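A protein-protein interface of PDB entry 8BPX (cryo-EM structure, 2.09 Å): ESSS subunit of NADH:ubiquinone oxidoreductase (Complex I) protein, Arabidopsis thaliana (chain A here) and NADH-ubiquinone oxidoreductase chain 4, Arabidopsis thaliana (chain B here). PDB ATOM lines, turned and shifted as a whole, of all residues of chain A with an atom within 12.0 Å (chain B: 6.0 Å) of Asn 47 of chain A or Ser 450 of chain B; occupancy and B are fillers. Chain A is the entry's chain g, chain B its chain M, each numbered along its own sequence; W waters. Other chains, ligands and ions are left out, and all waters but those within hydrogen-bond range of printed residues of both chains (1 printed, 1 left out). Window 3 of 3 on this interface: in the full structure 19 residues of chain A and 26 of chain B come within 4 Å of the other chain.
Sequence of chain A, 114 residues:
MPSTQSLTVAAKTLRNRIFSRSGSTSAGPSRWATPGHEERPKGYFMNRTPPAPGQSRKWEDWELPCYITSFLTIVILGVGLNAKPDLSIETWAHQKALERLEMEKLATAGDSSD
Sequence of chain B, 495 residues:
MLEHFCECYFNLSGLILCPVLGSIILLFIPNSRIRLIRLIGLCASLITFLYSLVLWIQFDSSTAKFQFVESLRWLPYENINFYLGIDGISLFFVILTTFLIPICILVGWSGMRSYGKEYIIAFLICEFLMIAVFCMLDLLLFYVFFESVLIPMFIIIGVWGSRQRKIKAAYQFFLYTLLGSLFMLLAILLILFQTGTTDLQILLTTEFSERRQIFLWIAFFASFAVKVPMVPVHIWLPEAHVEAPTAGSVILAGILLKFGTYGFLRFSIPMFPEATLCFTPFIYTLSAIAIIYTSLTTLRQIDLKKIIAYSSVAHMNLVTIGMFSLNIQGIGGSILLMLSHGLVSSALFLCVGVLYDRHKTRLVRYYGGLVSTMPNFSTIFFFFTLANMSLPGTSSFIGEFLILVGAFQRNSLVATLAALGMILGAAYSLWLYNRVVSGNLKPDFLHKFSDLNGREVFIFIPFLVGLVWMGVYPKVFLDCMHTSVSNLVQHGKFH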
ATOM      1  N   PRO A  41      16.786  -3.188  -8.930  1.00  0.00           N
ATOM      2  CA  PRO A  41      16.948  -4.308  -7.998  1.00  0.00           C
ATOM      3  C   PRO A  41      17.885  -5.378  -8.544  1.00  0.00           C
ATOM      4  O   PRO A  41      18.216  -5.412  -9.731  1.00  0.00           O
ATOM      5  CB  PRO A  41      15.523  -4.846  -7.845  1.00  0.00           C
ATOM      6  CG  PRO A  41      14.631  -3.723  -8.261  1.00  0.00           C
ATOM      7  CD  PRO A  41      15.383  -3.003  -9.334  1.00  0.00           C
ATOM      8  N   LYS A  42      18.285  -6.271  -7.631  1.00  0.00           N
ATOM      9  CA  LYS A  42      19.156  -7.408  -8.023  1.00  0.00           C
ATOM     10  C   LYS A  42      18.264  -8.533  -8.553  1.00  0.00           C
ATOM     11  O   LYS A  42      17.203  -8.786  -7.947  1.00  0.00           O
ATOM     12  CB  LYS A  42      20.030  -7.844  -6.840  1.00  0.00           C
ATOM     13  CG  LYS A  42      19.304  -8.111  -5.529  1.00  0.00           C
ATOM     14  CD  LYS A  42      20.136  -8.857  -4.509  1.00  0.00           C
ATOM     15  CE  LYS A  42      21.164  -7.999  -3.803  1.00  0.00           C
ATOM     16  NZ  LYS A  42      20.526  -7.025  -2.884  1.00  0.00           N
ATOM     17  N   GLY A  43      18.674  -9.170  -9.648  1.00  0.00           N
ATOM     18  CA  GLY A  43      17.901 -10.217 -10.280  1.00  0.00           C
ATOM     19  C   GLY A  43      16.811  -9.681 -11.190  1.00  0.00           C
ATOM     20  O   GLY A  43      16.608  -8.480 -11.353  1.00  0.00           O
ATOM     21  N   TYR A  44      16.092 -10.615 -11.799  1.00  0.00           N
ATOM     22  CA  TYR A  44      14.932 -10.299 -12.616  1.00  0.00           C
ATOM     23  C   TYR A  44      13.780 -11.158 -12.138  1.00  0.00           C
ATOM     24  O   TYR A  44      13.959 -12.355 -11.900  1.00  0.00           O
ATOM     25  CB  TYR A  44      15.208 -10.549 -14.100  1.00  0.00           C
ATOM     26  CG  TYR A  44      16.097  -9.495 -14.697  1.00  0.00           C
ATOM     27  CD1 TYR A  44      15.730  -8.162 -14.671  1.00  0.00           C
ATOM     28  CD2 TYR A  44      17.319  -9.831 -15.260  1.00  0.00           C
ATOM     29  CE1 TYR A  44      16.544  -7.194 -15.193  1.00  0.00           C
ATOM     30  CE2 TYR A  44      18.142  -8.864 -15.795  1.00  0.00           C
ATOM     31  CZ  TYR A  44      17.748  -7.548 -15.758  1.00  0.00           C
ATOM     32  OH  TYR A  44      18.558  -6.572 -16.288  1.00  0.00           O
ATOM     33  N   PHE A  45      12.610 -10.549 -11.989  1.00  0.00           N
ATOM     34  CA  PHE A  45      11.450 -11.286 -11.518  1.00  0.00           C
ATOM     35  C   PHE A  45      11.141 -12.446 -12.454  1.00  0.00           C
ATOM     36  O   PHE A  45      10.927 -12.246 -13.655  1.00  0.00           O
ATOM     37  CB  PHE A  45      10.246 -10.359 -11.398  1.00  0.00           C
ATOM     38  CG  PHE A  45       9.015 -11.049 -10.909  1.00  0.00           C
ATOM     39  CD1 PHE A  45       7.844 -11.017 -11.645  1.00  0.00           C
ATOM     40  CD2 PHE A  45       9.042 -11.766  -9.728  1.00  0.00           C
ATOM     41  CE1 PHE A  45       6.716 -11.666 -11.196  1.00  0.00           C
ATOM     42  CE2 PHE A  45       7.914 -12.421  -9.275  1.00  0.00           C
ATOM     43  CZ  PHE A  45       6.749 -12.371 -10.011  1.00  0.00           C
ATOM     44  N   MET A  46      11.120 -13.656 -11.899  1.00  0.00           N
ATOM     45  CA  MET A  46      10.919 -14.897 -12.647  1.00  0.00           C
ATOM     46  C   MET A  46      12.001 -15.131 -13.701  1.00  0.00           C
ATOM     47  O   MET A  46      11.769 -15.832 -14.687  1.00  0.00           O
ATOM     48  CB  MET A  46       9.511 -14.944 -13.258  1.00  0.00           C
ATOM     49  CG  MET A  46       8.432 -14.997 -12.176  1.00  0.00           C
ATOM     50  SD  MET A  46       6.719 -14.725 -12.666  1.00  0.00           S
ATOM     51  CE  MET A  46       6.930 -13.966 -14.261  1.00  0.00           C
ATOM     52  N   ASN A  47      13.185 -14.552 -13.483  1.00  0.00           N
ATOM     53  CA  ASN A  47      14.403 -14.850 -14.247  1.00  0.00           C
ATOM     54  C   ASN A  47      14.225 -14.646 -15.749  1.00  0.00           C
ATOM     55  O   ASN A  47      14.824 -15.350 -16.562  1.00  0.00           O
ATOM     56  CB  ASN A  47      14.906 -16.270 -13.961  1.00  0.00           C
ATOM     57  CG  ASN A  47      15.589 -16.397 -12.613  1.00  0.00           C
ATOM     58  OD1 ASN A  47      15.050 -15.966 -11.595  1.00  0.00           O
ATOM     59  ND2 ASN A  47      16.786 -16.972 -12.600  1.00  0.00           N
ATOM     60  N   ARG A  48      13.412 -13.670 -16.131  1.00  0.00           N
ATOM     61  CA  ARG A  48      13.265 -13.303 -17.534  1.00  0.00           C
ATOM     62  C   ARG A  48      13.955 -11.967 -17.770  1.00  0.00           C
ATOM     63  O   ARG A  48      13.724 -11.005 -17.037  1.00  0.00           O
ATOM     64  CB  ARG A  48      11.799 -13.231 -17.965  1.00  0.00           C
ATOM     65  CG  ARG A  48      10.885 -12.455 -17.043  1.00  0.00           C
ATOM     66  CD  ARG A  48       9.573 -12.129 -17.735  1.00  0.00           C
ATOM     67  NE  ARG A  48       8.649 -13.256 -17.776  1.00  0.00           N
ATOM     68  CZ  ARG A  48       7.367 -13.182 -17.447  1.00  0.00           C
ATOM     69  NH1 ARG A  48       6.828 -12.052 -17.015  1.00  0.00           N
ATOM     70  NH2 ARG A  48       6.612 -14.270 -17.534  1.00  0.00           N
ATOM     71  N   THR A  49      14.809 -11.919 -18.781  1.00  0.00           N
ATOM     72  CA  THR A  49      15.484 -10.681 -19.105  1.00  0.00           C
ATOM     73  C   THR A  49      14.479  -9.670 -19.654  1.00  0.00           C
ATOM     74  O   THR A  49      13.513 -10.044 -20.320  1.00  0.00           O
ATOM     75  CB  THR A  49      16.601 -10.924 -20.110  1.00  0.00           C
ATOM     76  OG1 THR A  49      16.065 -11.538 -21.287  1.00  0.00           O
ATOM     77  CG2 THR A  49      17.648 -11.836 -19.506  1.00  0.00           C
ATOM     78  N   PRO A  50      14.666  -8.384 -19.356  1.00  0.00           N
ATOM     79  CA  PRO A  50      13.691  -7.383 -19.793  1.00  0.00           C
ATOM     80  C   PRO A  50      13.683  -7.247 -21.304  1.00  0.00           C
ATOM     81  O   PRO A  50      14.669  -7.582 -21.979  1.00  0.00           O
ATOM     82  CB  PRO A  50      14.213  -6.113 -19.108  1.00  0.00           C
ATOM     83  CG  PRO A  50      15.674  -6.566 -19.278  1.00  0.00           C
ATOM     84  CD  PRO A  50      15.570  -7.668 -18.415  1.00  0.00           C
ATOM     85  N   PRO A  51      12.576  -6.799 -21.883  1.00  0.00           N
ATOM     86  CA  PRO A  51      12.547  -6.571 -23.332  1.00  0.00           C
ATOM     87  C   PRO A  51      13.402  -5.368 -23.700  1.00  0.00           C
ATOM     88  O   PRO A  51      13.776  -4.547 -22.861  1.00  0.00           O
ATOM     89  CB  PRO A  51      11.067  -6.340 -23.627  1.00  0.00           C
ATOM     90  CG  PRO A  51      10.506  -5.841 -22.347  1.00  0.00           C
ATOM     91  CD  PRO A  51      11.286  -6.487 -21.246  1.00  0.00           C
ATOM     92  N   ARG A  57       7.166  -7.287 -23.610  1.00  0.00           N
ATOM     93  CA  ARG A  57       7.433  -8.714 -23.518  1.00  0.00           C
ATOM     94  C   ARG A  57       6.423  -9.485 -24.360  1.00  0.00           C
ATOM     95  O   ARG A  57       5.237  -9.156 -24.395  1.00  0.00           O
ATOM     96  CB  ARG A  57       7.387  -9.171 -22.061  1.00  0.00           C
ATOM     97  CG  ARG A  57       7.486 -10.671 -21.886  1.00  0.00           C
ATOM     98  CD  ARG A  57       7.310 -11.093 -20.444  1.00  0.00           C
ATOM     99  NE  ARG A  57       5.925 -10.978 -20.008  1.00  0.00           N
ATOM    100  CZ  ARG A  57       5.055 -11.977 -20.009  1.00  0.00           C
ATOM    101  NH1 ARG A  57       5.373 -13.168 -20.481  1.00  0.00           N
ATOM    102  NH2 ARG A  57       3.829 -11.769 -19.536  1.00  0.00           N
ATOM    103  N   LYS A  58       6.911 -10.493 -25.075  1.00  0.00           N
ATOM    104  CA  LYS A  58       6.045 -11.338 -25.883  1.00  0.00           C
ATOM    105  C   LYS A  58       5.417 -12.389 -24.974  1.00  0.00           C
ATOM    106  O   LYS A  58       6.123 -13.077 -24.230  1.00  0.00           O
ATOM    107  CB  LYS A  58       6.865 -11.949 -27.028  1.00  0.00           C
ATOM    108  CG  LYS A  58       6.166 -12.834 -28.076  1.00  0.00           C
ATOM    109  CD  LYS A  58       7.031 -13.368 -29.211  1.00  0.00           C
ATOM    110  CE  LYS A  58       6.236 -14.249 -30.171  1.00  0.00           C
ATOM    111  NZ  LYS A  58       7.072 -14.777 -31.282  1.00  0.00           N
ATOM    112  N   GLU A  60       3.801 -15.810 -23.877  1.00  0.00           N
ATOM    113  CA  GLU A  60       3.787 -17.196 -24.321  1.00  0.00           C
ATOM    114  C   GLU A  60       2.356 -17.654 -24.592  1.00  0.00           C
ATOM    115  O   GLU A  60       1.384 -17.068 -24.112  1.00  0.00           O
ATOM    116  CB  GLU A  60       4.466 -18.102 -23.299  1.00  0.00           C
ATOM    117  CG  GLU A  60       5.875 -17.676 -22.940  1.00  0.00           C
ATOM    118  CD  GLU A  60       6.747 -18.837 -22.501  1.00  0.00           C
ATOM    119  OE1 GLU A  60       6.353 -19.555 -21.560  1.00  0.00           O
ATOM    120  OE2 GLU A  60       7.831 -19.028 -23.091  1.00  0.00           O
ATOM    121  N   TRP A  62       0.490 -20.043 -23.649  1.00  0.00           N
ATOM    122  CA  TRP A  62      -0.376 -20.477 -22.562  1.00  0.00           C
ATOM    123  C   TRP A  62      -0.934 -19.321 -21.739  1.00  0.00           C
ATOM    124  O   TRP A  62      -1.908 -19.520 -21.010  1.00  0.00           O
ATOM    125  CB  TRP A  62       0.383 -21.442 -21.643  1.00  0.00           C
ATOM    126  CG  TRP A  62       1.603 -20.824 -21.038  1.00  0.00           C
ATOM    127  CD1 TRP A  62       2.869 -20.863 -21.535  1.00  0.00           C
ATOM    128  CD2 TRP A  62       1.672 -20.053 -19.832  1.00  0.00           C
ATOM    129  NE1 TRP A  62       3.722 -20.172 -20.717  1.00  0.00           N
ATOM    130  CE2 TRP A  62       3.013 -19.665 -19.661  1.00  0.00           C
ATOM    131  CE3 TRP A  62       0.729 -19.661 -18.876  1.00  0.00           C
ATOM    132  CZ2 TRP A  62       3.437 -18.897 -18.583  1.00  0.00           C
ATOM    133  CZ3 TRP A  62       1.153 -18.902 -17.803  1.00  0.00           C
ATOM    134  CH2 TRP A  62       2.495 -18.528 -17.664  1.00  0.00           C
ATOM    135  N   GLU A  63      -0.354 -18.123 -21.854  1.00  0.00           N
ATOM    136  CA  GLU A  63      -0.630 -17.049 -20.900  1.00  0.00           C
ATOM    137  C   GLU A  63      -2.079 -16.580 -20.977  1.00  0.00           C
ATOM    138  O   GLU A  63      -2.794 -16.578 -19.972  1.00  0.00           O
ATOM    139  CB  GLU A  63       0.328 -15.883 -21.141  1.00  0.00           C
ATOM    140  CG  GLU A  63       1.792 -16.249 -20.967  1.00  0.00           C
ATOM    141  CD  GLU A  63       2.612 -15.145 -20.333  1.00  0.00           C
ATOM    142  OE1 GLU A  63       2.131 -14.499 -19.383  1.00  0.00           O
ATOM    143  OE2 GLU A  63       3.739 -14.914 -20.807  1.00  0.00           O
ATOM    144  N   ARG B 358      15.782 -29.475 -14.105  1.00  0.00           N
ATOM    145  CA  ARG B 358      17.019 -28.720 -14.264  1.00  0.00           C
ATOM    146  C   ARG B 358      18.249 -29.591 -14.026  1.00  0.00           C
ATOM    147  O   ARG B 358      19.208 -29.546 -14.803  1.00  0.00           O
ATOM    148  CB  ARG B 358      17.029 -27.523 -13.311  1.00  0.00           C
ATOM    149  CG  ARG B 358      15.905 -26.536 -13.554  1.00  0.00           C
ATOM    150  CD  ARG B 358      15.549 -25.765 -12.294  1.00  0.00           C
ATOM    151  NE  ARG B 358      14.864 -24.515 -12.594  1.00  0.00           N
ATOM    152  CZ  ARG B 358      13.617 -24.427 -13.033  1.00  0.00           C
ATOM    153  NH1 ARG B 358      12.868 -25.503 -13.211  1.00  0.00           N
ATOM    154  NH2 ARG B 358      13.106 -23.231 -13.295  1.00  0.00           N
ATOM    155  N   HIS B 359      18.244 -30.323 -12.922  1.00  0.00           N
ATOM    156  CA  HIS B 359      19.431 -31.022 -12.394  1.00  0.00           C
ATOM    157  C   HIS B 359      19.480 -32.527 -12.632  1.00  0.00           C
ATOM    158  O   HIS B 359      20.525 -33.040 -12.414  1.00  0.00           O
ATOM    159  CB  HIS B 359      19.615 -30.571 -10.911  1.00  0.00           C
ATOM    160  CG  HIS B 359      19.591 -29.090 -10.791  1.00  0.00           C
ATOM    161  ND1 HIS B 359      20.444 -28.293 -11.502  1.00  0.00           N
ATOM    162  CD2 HIS B 359      18.798 -28.261 -10.085  1.00  0.00           C
ATOM    163  CE1 HIS B 359      20.208 -27.040 -11.224  1.00  0.00           C
ATOM    164  NE2 HIS B 359      19.214 -26.993 -10.358  1.00  0.00           N
ATOM    165  N   THR B 373      20.085 -19.516  -4.185  1.00  0.00           N
ATOM    166  CA  THR B 373      19.980 -19.393  -5.632  1.00  0.00           C
ATOM    167  C   THR B 373      18.551 -19.453  -6.150  1.00  0.00           C
ATOM    168  O   THR B 373      18.290 -18.924  -7.231  1.00  0.00           O
ATOM    169  CB  THR B 373      20.808 -20.477  -6.349  1.00  0.00           C
ATOM    170  OG1 THR B 373      20.382 -21.785  -5.946  1.00  0.00           O
ATOM    171  CG2 THR B 373      22.290 -20.308  -6.048  1.00  0.00           C
ATOM    172  N   MET B 374      17.626 -20.073  -5.416  1.00  0.00           N
ATOM    173  CA  MET B 374      16.228 -20.193  -5.842  1.00  0.00           C
ATOM    174  C   MET B 374      15.285 -19.797  -4.709  1.00  0.00           C
ATOM    175  O   MET B 374      14.495 -20.613  -4.228  1.00  0.00           O
ATOM    176  CB  MET B 374      15.937 -21.615  -6.321  1.00  0.00           C
ATOM    177  CG  MET B 374      16.981 -22.213  -7.260  1.00  0.00           C
ATOM    178  SD  MET B 374      16.724 -23.964  -7.629  1.00  0.00           S
ATOM    179  CE  MET B 374      15.102 -23.961  -8.379  1.00  0.00           C
ATOM    180  N   ASN B 376      12.498 -18.035  -4.603  1.00  0.00           N
ATOM    181  CA  ASN B 376      11.069 -18.182  -4.873  1.00  0.00           C
ATOM    182  C   ASN B 376      10.638 -19.639  -4.752  1.00  0.00           C
ATOM    183  O   ASN B 376       9.638 -19.959  -4.087  1.00  0.00           O
ATOM    184  CB  ASN B 376      10.738 -17.638  -6.262  1.00  0.00           C
ATOM    185  CG  ASN B 376      10.677 -16.130  -6.295  1.00  0.00           C
ATOM    186  OD1 ASN B 376      10.375 -15.489  -5.293  1.00  0.00           O
ATOM    187  ND2 ASN B 376      10.968 -15.553  -7.448  1.00  0.00           N
ATOM    188  N   LYS B 448      25.224 -24.266 -11.437  1.00  0.00           N
ATOM    189  CA  LYS B 448      24.360 -23.460 -12.321  1.00  0.00           C
ATOM    190  C   LYS B 448      22.886 -23.605 -11.897  1.00  0.00           C
ATOM    191  O   LYS B 448      22.425 -24.678 -11.766  1.00  0.00           O
ATOM    192  CB  LYS B 448      24.737 -23.747 -13.774  1.00  0.00           C
ATOM    193  CG  LYS B 448      23.909 -23.123 -14.867  1.00  0.00           C
ATOM    194  CD  LYS B 448      24.424 -23.526 -16.232  1.00  0.00           C
ATOM    195  CE  LYS B 448      25.831 -23.043 -16.485  1.00  0.00           C
ATOM    196  NZ  LYS B 448      25.845 -21.588 -16.768  1.00  0.00           N
ATOM    197  N   PHE B 449      22.199 -22.489 -11.752  1.00  0.00           N
ATOM    198  CA  PHE B 449      20.839 -22.492 -11.164  1.00  0.00           C
ATOM    199  C   PHE B 449      19.903 -21.528 -11.882  1.00  0.00           C
ATOM    200  O   PHE B 449      20.306 -20.589 -12.472  1.00  0.00           O
ATOM    201  CB  PHE B 449      20.863 -22.286  -9.622  1.00  0.00           C
ATOM    202  CG  PHE B 449      21.799 -23.150  -8.834  1.00  0.00           C
ATOM    203  CD1 PHE B 449      23.124 -22.789  -8.674  1.00  0.00           C
ATOM    204  CD2 PHE B 449      21.340 -24.306  -8.230  1.00  0.00           C
ATOM    205  CE1 PHE B 449      23.982 -23.591  -7.945  1.00  0.00           C
ATOM    206  CE2 PHE B 449      22.201 -25.099  -7.499  1.00  0.00           C
ATOM    207  CZ  PHE B 449      23.516 -24.741  -7.358  1.00  0.00           C
ATOM    208  N   SER B 450      18.630 -21.827 -11.791  1.00  0.00           N
ATOM    209  CA  SER B 450      17.578 -20.956 -12.297  1.00  0.00           C
ATOM    210  C   SER B 450      16.364 -21.087 -11.394  1.00  0.00           C
ATOM    211  O   SER B 450      15.895 -22.201 -11.147  1.00  0.00           O
ATOM    212  CB  SER B 450      17.202 -21.311 -13.738  1.00  0.00           C
ATOM    213  OG  SER B 450      16.477 -20.260 -14.338  1.00  0.00           O
ATOM    214  N   ASP B 451      15.859 -19.955 -10.908  1.00  0.00           N
ATOM    215  CA  ASP B 451      14.615 -19.952 -10.155  1.00  0.00           C
ATOM    216  C   ASP B 451      13.439 -20.188 -11.104  1.00  0.00           C
ATOM    217  O   ASP B 451      13.602 -20.391 -12.307  1.00  0.00           O
ATOM    218  CB  ASP B 451      14.460 -18.642  -9.380  1.00  0.00           C
ATOM    219  CG  ASP B 451      13.834 -18.841  -7.998  1.00  0.00           C
ATOM    220  OD1 ASP B 451      13.191 -19.881  -7.762  1.00  0.00           O
ATOM    221  OD2 ASP B 451      13.977 -17.945  -7.148  1.00  0.00           O
ATOM    222  N   LEU B 452      12.231 -20.155 -10.550  1.00  0.00           N
ATOM    223  CA  LEU B 452      11.041 -20.472 -11.325  1.00  0.00           C
ATOM    224  C   LEU B 452      10.792 -19.445 -12.423  1.00  0.00           C
ATOM    225  O   LEU B 452      10.967 -18.242 -12.223  1.00  0.00           O
ATOM    226  CB  LEU B 452       9.824 -20.560 -10.409  1.00  0.00           C
ATOM    227  CG  LEU B 452      10.034 -21.292  -9.082  1.00  0.00           C
ATOM    228  CD1 LEU B 452       8.930 -20.939  -8.109  1.00  0.00           C
ATOM    229  CD2 LEU B 452      10.113 -22.798  -9.296  1.00  0.00           C
ATOM    230  N   ASN B 453      10.381 -19.932 -13.593  1.00  0.00           N
ATOM    231  CA  ASN B 453       9.919 -19.050 -14.650  1.00  0.00           C
ATOM    232  C   ASN B 453       8.438 -18.729 -14.439  1.00  0.00           C
ATOM    233  O   ASN B 453       7.802 -19.197 -13.492  1.00  0.00           O
ATOM    234  CB  ASN B 453      10.160 -19.666 -16.032  1.00  0.00           C
ATOM    235  CG  ASN B 453       9.646 -21.089 -16.152  1.00  0.00           C
ATOM    236  OD1 ASN B 453       8.500 -21.382 -15.826  1.00  0.00           O
ATOM    237  ND2 ASN B 453      10.490 -21.974 -16.652  1.00  0.00           N
HETATM  238  O   HOH W   1      17.671 -16.428  -9.286  1.00  0.00           O
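NE of Arg 358 of chain B is in hydrogen-bond range of O of Ser 450 of chain B (2.9 Å). The backbone carbonyl oxygen (O) of Asp 451 of chain B sits at hydrogen-bond distance from the guanidinium group (NH2) of Arg 358 of chain B (3.0 Å). N of Asn 376 of chain B sits at hydrogen-bond distance from OD2 of Asp 451 of chain B (2.9 Å).
Water W1 lies within hydrogen-bond range of O of Thr 373 of chain B (3.3 Å) and ND2 of Asn 47 of chain A (3.5 Å).
Met 46 of chain A touches Leu 452 of chain B (CA to O, 3.4 Å). Asn 453 of chain B touches Met 46 of chain A (CA to O, 3.7 Å). Asn 47 of chain A touches Ser 450 of chain B (ND2 to OG, 3.7 Å). Asp 451 of chain B touches Asn 47 of chain A.
Of the 11 printed residues of chain B, 4 touch a printed residue of chain A. Printed residues of chain A that touch a printed residue of chain B: Met 46 and Asn 47. Hydrophobic or aromatic side chains of chain A within 4 Å of the printed part of chain B: Met 46. Among the printed residues, 4 pairs touch across the chains.
Printed residues of chain B within 4 Å of Asn 47 of chain A: Ser 450 (3.7 Å) and Asp 451 (3.5 Å). No residue of chain A comes within 4 Å of Met 374 of chain B. No residue of chain A comes within 4 Å of Phe 449 of chain B. Leu 452 of chain B touches just one residue of chain A: Met 46. Printed residues of chain B within 4 Å of Met 46 of chain A: Leu 452 (3.4 Å) and Asn 453 (3.7 Å). Printed residues of chain A within 4 Å of Asn 453 of chain B: Met 46 (3.7 Å). Pro 50 of chain A touches none of the printed residues of chain B. The nearest printed residue of chain B that does not touch Met 46 of chain A is Asn 376 of chain B (4.8 Å).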
